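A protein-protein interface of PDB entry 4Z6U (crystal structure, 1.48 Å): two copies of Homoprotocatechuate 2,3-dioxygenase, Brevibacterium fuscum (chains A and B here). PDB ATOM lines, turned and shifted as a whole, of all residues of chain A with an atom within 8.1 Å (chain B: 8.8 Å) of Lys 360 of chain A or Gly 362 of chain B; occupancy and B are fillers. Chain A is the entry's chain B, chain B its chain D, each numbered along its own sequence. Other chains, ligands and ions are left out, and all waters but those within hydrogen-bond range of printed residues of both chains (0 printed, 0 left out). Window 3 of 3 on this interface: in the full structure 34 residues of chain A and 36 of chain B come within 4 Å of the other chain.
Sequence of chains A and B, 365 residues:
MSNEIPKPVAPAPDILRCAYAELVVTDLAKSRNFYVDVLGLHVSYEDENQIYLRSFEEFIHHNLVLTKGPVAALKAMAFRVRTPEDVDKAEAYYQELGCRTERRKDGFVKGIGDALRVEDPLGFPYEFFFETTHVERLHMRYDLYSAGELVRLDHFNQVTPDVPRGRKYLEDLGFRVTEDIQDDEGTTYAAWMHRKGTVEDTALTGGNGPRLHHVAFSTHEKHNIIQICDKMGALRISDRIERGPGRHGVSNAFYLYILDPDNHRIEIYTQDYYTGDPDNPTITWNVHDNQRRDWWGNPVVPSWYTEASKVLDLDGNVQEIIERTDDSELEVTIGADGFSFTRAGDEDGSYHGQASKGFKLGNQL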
ATOM      1  N   PRO A 299     -22.826  14.028 -20.253  1.00  0.00           N
ATOM      2  CA  PRO A 299     -22.795  13.023 -19.213  1.00  0.00           C
ATOM      3  C   PRO A 299     -21.348  12.607 -18.910  1.00  0.00           C
ATOM      4  O   PRO A 299     -20.477  12.634 -19.783  1.00  0.00           O
ATOM      5  CB  PRO A 299     -23.601  11.862 -19.817  1.00  0.00           C
ATOM      6  CG  PRO A 299     -23.431  12.019 -21.273  1.00  0.00           C
ATOM      7  CD  PRO A 299     -23.415  13.502 -21.496  1.00  0.00           C
ATOM      8  N   PRO A 302     -19.016   6.473 -17.038  1.00  0.00           N
ATOM      9  CA  PRO A 302     -18.890   5.753 -15.771  1.00  0.00           C
ATOM     10  C   PRO A 302     -17.444   5.370 -15.413  1.00  0.00           C
ATOM     11  O   PRO A 302     -17.083   5.413 -14.263  1.00  0.00           O
ATOM     12  CB  PRO A 302     -19.783   4.531 -15.937  1.00  0.00           C
ATOM     13  CG  PRO A 302     -20.698   4.877 -17.086  1.00  0.00           C
ATOM     14  CD  PRO A 302     -19.987   5.852 -17.956  1.00  0.00           C
ATOM     15  N   ILE A 334     -26.046   9.313 -11.791  1.00  0.00           N
ATOM     16  CA  ILE A 334     -26.351   8.597 -13.026  1.00  0.00           C
ATOM     17  C   ILE A 334     -26.725   7.134 -12.829  1.00  0.00           C
ATOM     18  O   ILE A 334     -27.044   6.447 -13.817  1.00  0.00           O
ATOM     19  CB  ILE A 334     -25.204   8.730 -14.079  1.00  0.00           C
ATOM     20  CG1 ILE A 334     -23.913   8.080 -13.577  1.00  0.00           C
ATOM     21  CG2 ILE A 334     -24.965  10.210 -14.385  1.00  0.00           C
ATOM     22  CD1 ILE A 334     -22.747   8.125 -14.583  1.00  0.00           C
ATOM     23  N   GLY A 335     -26.686   6.660 -11.581  1.00  0.00           N
ATOM     24  CA  GLY A 335     -27.054   5.290 -11.277  1.00  0.00           C
ATOM     25  C   GLY A 335     -28.561   5.111 -11.234  1.00  0.00           C
ATOM     26  O   GLY A 335     -29.330   6.036 -11.501  1.00  0.00           O
ATOM     27  N   ALA A 336     -28.989   3.925 -10.853  1.00  0.00           N
ATOM     28  CA  ALA A 336     -30.418   3.533 -10.946  1.00  0.00           C
ATOM     29  C   ALA A 336     -31.323   4.431 -10.135  1.00  0.00           C
ATOM     30  O   ALA A 336     -32.450   4.680 -10.522  1.00  0.00           O
ATOM     31  CB  ALA A 336     -30.569   2.106 -10.468  1.00  0.00           C
ATOM     32  N   HIS A 352     -33.654  11.332 -14.007  1.00  0.00           N
ATOM     33  CA  HIS A 352     -33.967  10.395 -12.951  1.00  0.00           C
ATOM     34  C   HIS A 352     -33.496   9.008 -13.368  1.00  0.00           C
ATOM     35  O   HIS A 352     -33.948   8.471 -14.386  1.00  0.00           O
ATOM     36  CB  HIS A 352     -35.476  10.351 -12.717  1.00  0.00           C
ATOM     37  CG  HIS A 352     -36.063  11.668 -12.326  1.00  0.00           C
ATOM     38  ND1 HIS A 352     -36.365  11.987 -11.019  1.00  0.00           N
ATOM     39  CD2 HIS A 352     -36.420  12.742 -13.071  1.00  0.00           C
ATOM     40  CE1 HIS A 352     -36.883  13.202 -10.977  1.00  0.00           C
ATOM     41  NE2 HIS A 352     -36.932  13.677 -12.210  1.00  0.00           N
ATOM     42  N   GLY A 353     -32.558   8.459 -12.604  1.00  0.00           N
ATOM     43  CA  GLY A 353     -32.050   7.095 -12.838  1.00  0.00           C
ATOM     44  C   GLY A 353     -31.345   6.885 -14.166  1.00  0.00           C
ATOM     45  O   GLY A 353     -31.328   5.765 -14.698  1.00  0.00           O
ATOM     46  N   GLN A 354     -30.770   7.952 -14.719  1.00  0.00           N
ATOM     47  CA  GLN A 354     -29.997   7.830 -15.942  1.00  0.00           C
ATOM     48  C   GLN A 354     -29.151   9.068 -16.153  1.00  0.00           C
ATOM     49  O   GLN A 354     -29.292  10.054 -15.426  1.00  0.00           O
ATOM     50  CB  GLN A 354     -30.897   7.544 -17.165  1.00  0.00           C
ATOM     51  CG  GLN A 354     -31.455   8.737 -17.926  1.00  0.00           C
ATOM     52  CD  GLN A 354     -32.149   8.304 -19.224  1.00  0.00           C
ATOM     53  OE1 GLN A 354     -33.092   7.509 -19.189  1.00  0.00           O
ATOM     54  NE2 GLN A 354     -31.674   8.808 -20.375  1.00  0.00           N
ATOM     55  N   ALA A 355     -28.262   8.997 -17.136  1.00  0.00           N
ATOM     56  CA  ALA A 355     -27.377  10.090 -17.427  1.00  0.00           C
ATOM     57  C   ALA A 355     -28.090  11.128 -18.308  1.00  0.00           C
ATOM     58  O   ALA A 355     -29.202  10.890 -18.806  1.00  0.00           O
ATOM     59  CB  ALA A 355     -26.120   9.558 -18.091  1.00  0.00           C
ATOM     60  N   SER A 356     -27.468  12.296 -18.455  1.00  0.00           N
ATOM     61  CA  SER A 356     -27.978  13.331 -19.379  1.00  0.00           C
ATOM     62  C   SER A 356     -27.888  12.934 -20.845  1.00  0.00           C
ATOM     63  O   SER A 356     -27.198  11.942 -21.220  1.00  0.00           O
ATOM     64  CB  SER A 356     -27.211  14.629 -19.148  1.00  0.00           C
ATOM     65  OG  SER A 356     -25.839  14.391 -19.298  1.00  0.00           O
ATOM     66  N   LYS A 357     -28.565  13.718 -21.683  1.00  0.00           N
ATOM     67  CA  LYS A 357     -28.425  13.644 -23.142  1.00  0.00           C
ATOM     68  C   LYS A 357     -28.820  12.306 -23.732  1.00  0.00           C
ATOM     69  O   LYS A 357     -28.363  11.958 -24.811  1.00  0.00           O
ATOM     70  CB  LYS A 357     -26.999  14.059 -23.604  1.00  0.00           C
ATOM     71  CG  LYS A 357     -26.468  15.280 -22.859  1.00  0.00           C
ATOM     72  CD  LYS A 357     -26.486  16.535 -23.672  1.00  0.00           C
ATOM     73  CE  LYS A 357     -25.755  17.718 -23.080  1.00  0.00           C
ATOM     74  NZ  LYS A 357     -26.664  18.864 -22.774  1.00  0.00           N
ATOM     75  N   GLY A 358     -29.681  11.554 -23.052  1.00  0.00           N
ATOM     76  CA  GLY A 358     -30.299  10.398 -23.701  1.00  0.00           C
ATOM     77  C   GLY A 358     -29.579   9.073 -23.463  1.00  0.00           C
ATOM     78  O   GLY A 358     -29.932   8.062 -24.076  1.00  0.00           O
ATOM     79  N   PHE A 359     -28.613   9.072 -22.545  1.00  0.00           N
ATOM     80  CA  PHE A 359     -27.822   7.876 -22.223  1.00  0.00           C
ATOM     81  C   PHE A 359     -28.096   7.264 -20.838  1.00  0.00           C
ATOM     82  O   PHE A 359     -28.534   7.939 -19.916  1.00  0.00           O
ATOM     83  CB  PHE A 359     -26.341   8.197 -22.369  1.00  0.00           C
ATOM     84  CG  PHE A 359     -25.945   8.537 -23.771  1.00  0.00           C
ATOM     85  CD1 PHE A 359     -26.035   7.600 -24.781  1.00  0.00           C
ATOM     86  CD2 PHE A 359     -25.478   9.819 -24.080  1.00  0.00           C
ATOM     87  CE1 PHE A 359     -25.653   7.938 -26.085  1.00  0.00           C
ATOM     88  CE2 PHE A 359     -25.097  10.146 -25.360  1.00  0.00           C
ATOM     89  CZ  PHE A 359     -25.200   9.199 -26.363  1.00  0.00           C
ATOM     90  N   LYS A 360     -27.831   5.962 -20.746  1.00  0.00           N
ATOM     91  CA  LYS A 360     -27.813   5.198 -19.506  1.00  0.00           C
ATOM     92  C   LYS A 360     -26.470   4.535 -19.377  1.00  0.00           C
ATOM     93  O   LYS A 360     -25.766   4.379 -20.383  1.00  0.00           O
ATOM     94  CB  LYS A 360     -28.883   4.091 -19.529  1.00  0.00           C
ATOM     95  CG  LYS A 360     -30.154   4.459 -18.850  1.00  0.00           C
ATOM     96  CD  LYS A 360     -31.121   3.289 -18.916  1.00  0.00           C
ATOM     97  CE  LYS A 360     -32.374   3.586 -18.093  1.00  0.00           C
ATOM     98  NZ  LYS A 360     -33.616   3.314 -18.871  1.00  0.00           N
ATOM     99  N   LEU A 361     -26.117   4.161 -18.145  1.00  0.00           N
ATOM    100  CA  LEU A 361     -24.944   3.312 -17.875  1.00  0.00           C
ATOM    101  C   LEU A 361     -24.944   2.050 -18.769  1.00  0.00           C
ATOM    102  O   LEU A 361     -25.972   1.368 -18.865  1.00  0.00           O
ATOM    103  CB  LEU A 361     -24.941   2.850 -16.404  1.00  0.00           C
ATOM    104  CG  LEU A 361     -24.764   3.791 -15.210  1.00  0.00           C
ATOM    105  CD1 LEU A 361     -25.218   3.083 -13.938  1.00  0.00           C
ATOM    106  CD2 LEU A 361     -23.319   4.179 -15.077  1.00  0.00           C
ATOM    107  N   GLY A 362     -23.813   1.722 -19.416  1.00  0.00           N
ATOM    108  CA  GLY A 362     -23.692   0.416 -20.109  1.00  0.00           C
ATOM    109  C   GLY A 362     -23.814  -0.776 -19.156  1.00  0.00           C
ATOM    110  O   GLY A 362     -23.512  -0.642 -17.963  1.00  0.00           O
ATOM    111  N   VAL B 301     -26.164  10.923 -29.809  1.00  0.00           N
ATOM    112  CA  VAL B 301     -27.333  10.823 -28.932  1.00  0.00           C
ATOM    113  C   VAL B 301     -28.546  10.338 -29.738  1.00  0.00           C
ATOM    114  O   VAL B 301     -28.749  10.719 -30.900  1.00  0.00           O
ATOM    115  CB  VAL B 301     -27.623  12.163 -28.246  1.00  0.00           C
ATOM    116  CG1 VAL B 301     -26.376  12.712 -27.537  1.00  0.00           C
ATOM    117  CG2 VAL B 301     -28.107  13.199 -29.232  1.00  0.00           C
ATOM    118  N   PRO B 302     -29.328   9.432 -29.173  1.00  0.00           N
ATOM    119  CA  PRO B 302     -30.403   8.801 -29.971  1.00  0.00           C
ATOM    120  C   PRO B 302     -31.423   9.797 -30.573  1.00  0.00           C
ATOM    121  O   PRO B 302     -31.910   9.571 -31.692  1.00  0.00           O
ATOM    122  CB  PRO B 302     -31.050   7.827 -28.989  1.00  0.00           C
ATOM    123  CG  PRO B 302     -30.023   7.600 -27.942  1.00  0.00           C
ATOM    124  CD  PRO B 302     -29.174   8.811 -27.841  1.00  0.00           C
ATOM    125  N   SER B 303     -31.707  10.888 -29.856  1.00  0.00           N
ATOM    126  CA  SER B 303     -32.617  11.929 -30.357  1.00  0.00           C
ATOM    127  C   SER B 303     -32.136  12.498 -31.684  1.00  0.00           C
ATOM    128  O   SER B 303     -32.958  12.941 -32.506  1.00  0.00           O
ATOM    129  CB  SER B 303     -32.768  13.077 -29.356  1.00  0.00           C
ATOM    130  OG  SER B 303     -31.542  13.791 -29.120  1.00  0.00           O
ATOM    131  N   ILE B 334     -25.746   1.712 -32.495  1.00  0.00           N
ATOM    132  CA  ILE B 334     -25.799   1.922 -31.040  1.00  0.00           C
ATOM    133  C   ILE B 334     -26.974   1.226 -30.337  1.00  0.00           C
ATOM    134  O   ILE B 334     -27.060   1.270 -29.094  1.00  0.00           O
ATOM    135  CB  ILE B 334     -25.792   3.419 -30.651  1.00  0.00           C
ATOM    136  CG1 ILE B 334     -27.003   4.169 -31.228  1.00  0.00           C
ATOM    137  CG2 ILE B 334     -24.517   4.104 -31.134  1.00  0.00           C
ATOM    138  CD1 ILE B 334     -27.171   5.590 -30.685  1.00  0.00           C
ATOM    139  N   GLN B 354     -24.113  -1.280 -27.602  1.00  0.00           N
ATOM    140  CA  GLN B 354     -24.176  -0.022 -26.920  1.00  0.00           C
ATOM    141  C   GLN B 354     -23.373   1.011 -27.691  1.00  0.00           C
ATOM    142  O   GLN B 354     -22.771   0.706 -28.746  1.00  0.00           O
ATOM    143  CB  GLN B 354     -23.677  -0.144 -25.493  1.00  0.00           C
ATOM    144  CG  GLN B 354     -22.255  -0.638 -25.302  1.00  0.00           C
ATOM    145  CD  GLN B 354     -21.993  -0.864 -23.813  1.00  0.00           C
ATOM    146  OE1 GLN B 354     -22.724  -1.589 -23.183  1.00  0.00           O
ATOM    147  NE2 GLN B 354     -21.048  -0.143 -23.238  1.00  0.00           N
ATOM    148  N   ALA B 355     -23.408   2.231 -27.187  1.00  0.00           N
ATOM    149  CA  ALA B 355     -22.684   3.304 -27.814  1.00  0.00           C
ATOM    150  C   ALA B 355     -21.241   3.291 -27.310  1.00  0.00           C
ATOM    151  O   ALA B 355     -20.864   2.475 -26.432  1.00  0.00           O
ATOM    152  CB  ALA B 355     -23.398   4.617 -27.545  1.00  0.00           C
ATOM    153  N   SER B 356     -20.426   4.159 -27.888  1.00  0.00           N
ATOM    154  CA  SER B 356     -19.058   4.362 -27.440  1.00  0.00           C
ATOM    155  C   SER B 356     -19.020   4.967 -26.032  1.00  0.00           C
ATOM    156  O   SER B 356     -20.037   5.483 -25.525  1.00  0.00           O
ATOM    157  CB  SER B 356     -18.317   5.248 -28.452  1.00  0.00           C
ATOM    158  OG  SER B 356     -19.068   6.439 -28.649  1.00  0.00           O
ATOM    159  N   LYS B 357     -17.825   4.919 -25.427  1.00  0.00           N
ATOM    160  CA  LYS B 357     -17.473   5.667 -24.219  1.00  0.00           C
ATOM    161  C   LYS B 357     -18.186   5.164 -22.961  1.00  0.00           C
ATOM    162  O   LYS B 357     -18.072   5.777 -21.905  1.00  0.00           O
ATOM    163  CB  LYS B 357     -17.648   7.218 -24.360  1.00  0.00           C
ATOM    164  CG  LYS B 357     -17.145   7.894 -25.646  1.00  0.00           C
ATOM    165  CD  LYS B 357     -15.654   7.914 -25.842  1.00  0.00           C
ATOM    166  CE  LYS B 357     -15.197   8.788 -27.012  1.00  0.00           C
ATOM    167  NZ  LYS B 357     -13.893   8.278 -27.561  1.00  0.00           N
ATOM    168  N   GLY B 358     -18.910   4.048 -23.044  1.00  0.00           N
ATOM    169  CA  GLY B 358     -19.435   3.395 -21.839  1.00  0.00           C
ATOM    170  C   GLY B 358     -20.924   3.576 -21.596  1.00  0.00           C
ATOM    171  O   GLY B 358     -21.452   3.177 -20.540  1.00  0.00           O
ATOM    172  N   PHE B 359     -21.618   4.168 -22.560  1.00  0.00           N
ATOM    173  CA  PHE B 359     -23.058   4.388 -22.451  1.00  0.00           C
ATOM    174  C   PHE B 359     -23.876   3.403 -23.289  1.00  0.00           C
ATOM    175  O   PHE B 359     -23.437   2.941 -24.349  1.00  0.00           O
ATOM    176  CB  PHE B 359     -23.389   5.809 -22.931  1.00  0.00           C
ATOM    177  CG  PHE B 359     -22.763   6.888 -22.116  1.00  0.00           C
ATOM    178  CD1 PHE B 359     -23.163   7.091 -20.810  1.00  0.00           C
ATOM    179  CD2 PHE B 359     -21.784   7.721 -22.675  1.00  0.00           C
ATOM    180  CE1 PHE B 359     -22.578   8.094 -20.049  1.00  0.00           C
ATOM    181  CE2 PHE B 359     -21.208   8.724 -21.922  1.00  0.00           C
ATOM    182  CZ  PHE B 359     -21.612   8.909 -20.609  1.00  0.00           C
ATOM    183  N   LYS B 360     -25.093   3.130 -22.834  1.00  0.00           N
ATOM    184  CA  LYS B 360     -26.109   2.554 -23.703  1.00  0.00           C
ATOM    185  C   LYS B 360     -27.284   3.502 -23.848  1.00  0.00           C
ATOM    186  O   LYS B 360     -27.321   4.585 -23.224  1.00  0.00           O
ATOM    187  CB  LYS B 360     -26.531   1.187 -23.178  1.00  0.00           C
ATOM    188  CG  LYS B 360     -27.399   1.252 -21.948  1.00  0.00           C
ATOM    189  CD  LYS B 360     -27.885  -0.112 -21.534  1.00  0.00           C
ATOM    190  CE  LYS B 360     -28.867   0.033 -20.384  1.00  0.00           C
ATOM    191  NZ  LYS B 360     -29.314  -1.293 -19.903  1.00  0.00           N
ATOM    192  N   LEU B 361     -28.250   3.108 -24.675  1.00  0.00           N
ATOM    193  CA  LEU B 361     -29.384   3.983 -24.954  1.00  0.00           C
ATOM    194  C   LEU B 361     -30.172   4.143 -23.677  1.00  0.00           C
ATOM    195  O   LEU B 361     -30.436   3.172 -22.971  1.00  0.00           O
ATOM    196  CB  LEU B 361     -30.304   3.418 -26.040  1.00  0.00           C
ATOM    197  CG  LEU B 361     -29.697   3.049 -27.387  1.00  0.00           C
ATOM    198  CD1 LEU B 361     -30.782   2.422 -28.258  1.00  0.00           C
ATOM    199  CD2 LEU B 361     -29.073   4.240 -28.060  1.00  0.00           C
ATOM    200  N   GLY B 362     -30.561   5.383 -23.406  1.00  0.00           N
ATOM    201  CA  GLY B 362     -31.415   5.714 -22.265  1.00  0.00           C
ATOM    202  C   GLY B 362     -32.884   5.494 -22.562  1.00  0.00           C
ATOM    203  O   GLY B 362     -33.204   4.900 -23.603  1.00  0.00           O
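The backbone carbonyl oxygen (O) of Gly 358 of chain B lies within hydrogen-bond range of the backbone NH (N) of Gly 362 of chain A, at 3.0 Å.
The backbone carbonyl oxygen of Gly 358 of chain A sits at hydrogen-bond distance from the backbone NH of Gly 362 of chain B (2.8 Å).
The backbone carbonyl oxygen of Lys 360 of chain A sits at hydrogen-bond distance from the backbone NH of Lys 360 of chain B, at 2.8 Å.
O of Phe 359 of chain A is in hydrogen-bond range of NE2 of Gln 354 of chain A (3.3 Å).
Pro 302 of chain A touches Gly 358 of chain B.
Val 301 of chain B touches Lys 357 of chain A (CG1 to O, 3.5 Å).
Gly 358 of chain A touches Leu 361 of chain B (O to C, 3.9 Å).
CG1 of Val 301 of chain B touches CE2 of Phe 359 of chain A, 3.6 Å away.
CA of Phe 359 of chain A touches N of Gly 362 of chain B, at 3.9 Å.
Phe 359 of chain B touches Lys 360 of chain A.
Lys 360 of chain A touches Leu 361 of chain B (CB to O, 3.9 Å).
CG of Lys 360 of chain B touches O of Leu 361 of chain A, 3.4 Å away.
Gln 354 of chain B touches Gly 362 of chain A.
Lys 360 of chain B touches Gly 362 of chain A (N to N, 3.9 Å).
His 352 of chain A touches none of the printed residues of chain B.
Printed residues of chain B within 4 Å of Lys 357 of chain A: Val 301 (3.5 Å).
Of chain B, only Phe 359, Lys 360, Leu 361 and Gly 362 come within 4 Å of Lys 360 of chain A.
Printed residues of chain A within 4 Å of Gln 354 of chain B: Gly 362 (3.8 Å).
Of the printed residues of chain A, Gly 358 of chain B touches Pro 302 and Gly 362.
Of the printed residues of chain A, Lys 360 of chain B touches Phe 359, Lys 360, Leu 361 and Gly 362.
Printed residues of chain A within 4 Å of Gly 362 of chain B: Gln 354 (3.6 Å), Gly 358 (2.8 Å), Phe 359 (3.9 Å) and Lys 360 (3.9 Å).
The nearest printed residue of chain A that does not touch Gly 362 of chain B is Ala 355 of chain A (6.6 Å).
The nearest printed residue of chain B that does not touch Pro 302 of chain A is Phe 359 of chain B (4.02 Å).
Of the 16 printed residues of chain A, 9 touch a printed residue of chain B.
Hydrophobic or aromatic side chains of chain A within 4 Å of the printed part of chain B: Pro 299, Pro 302 and Phe 359.
Along chain A the printed residues that touch a printed residue of chain B span positions 299 to 362.
Hydrophobic or aromatic side chains of chain B within 4 Å of the printed part of chain A: Val 301, Pro 302 and Phe 359.
Among the printed residues, 19 pairs touch across the chains.
Among the printed residues, no Asp or Glu carboxylate lies within 4 Å of a Lys or Arg side-chain nitrogen of the other chain.
Gly 358 of chain A touches Gly 362 of chain B, and with the chains exchanged Gly 362 of chain A touches Gly 358 of chain B.
Phe 359 of chain A touches its own counterpart, Phe 359 of chain B.
Phe 359 of chain A touches Gly 362 of chain B, but with the chains exchanged Gly 362 of chain A does not touch Phe 359 of chain B (4.1 Å).
Lys 360 of chain A touches its own counterpart, Lys 360 of chain B.
11 positions are printed for both chains.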
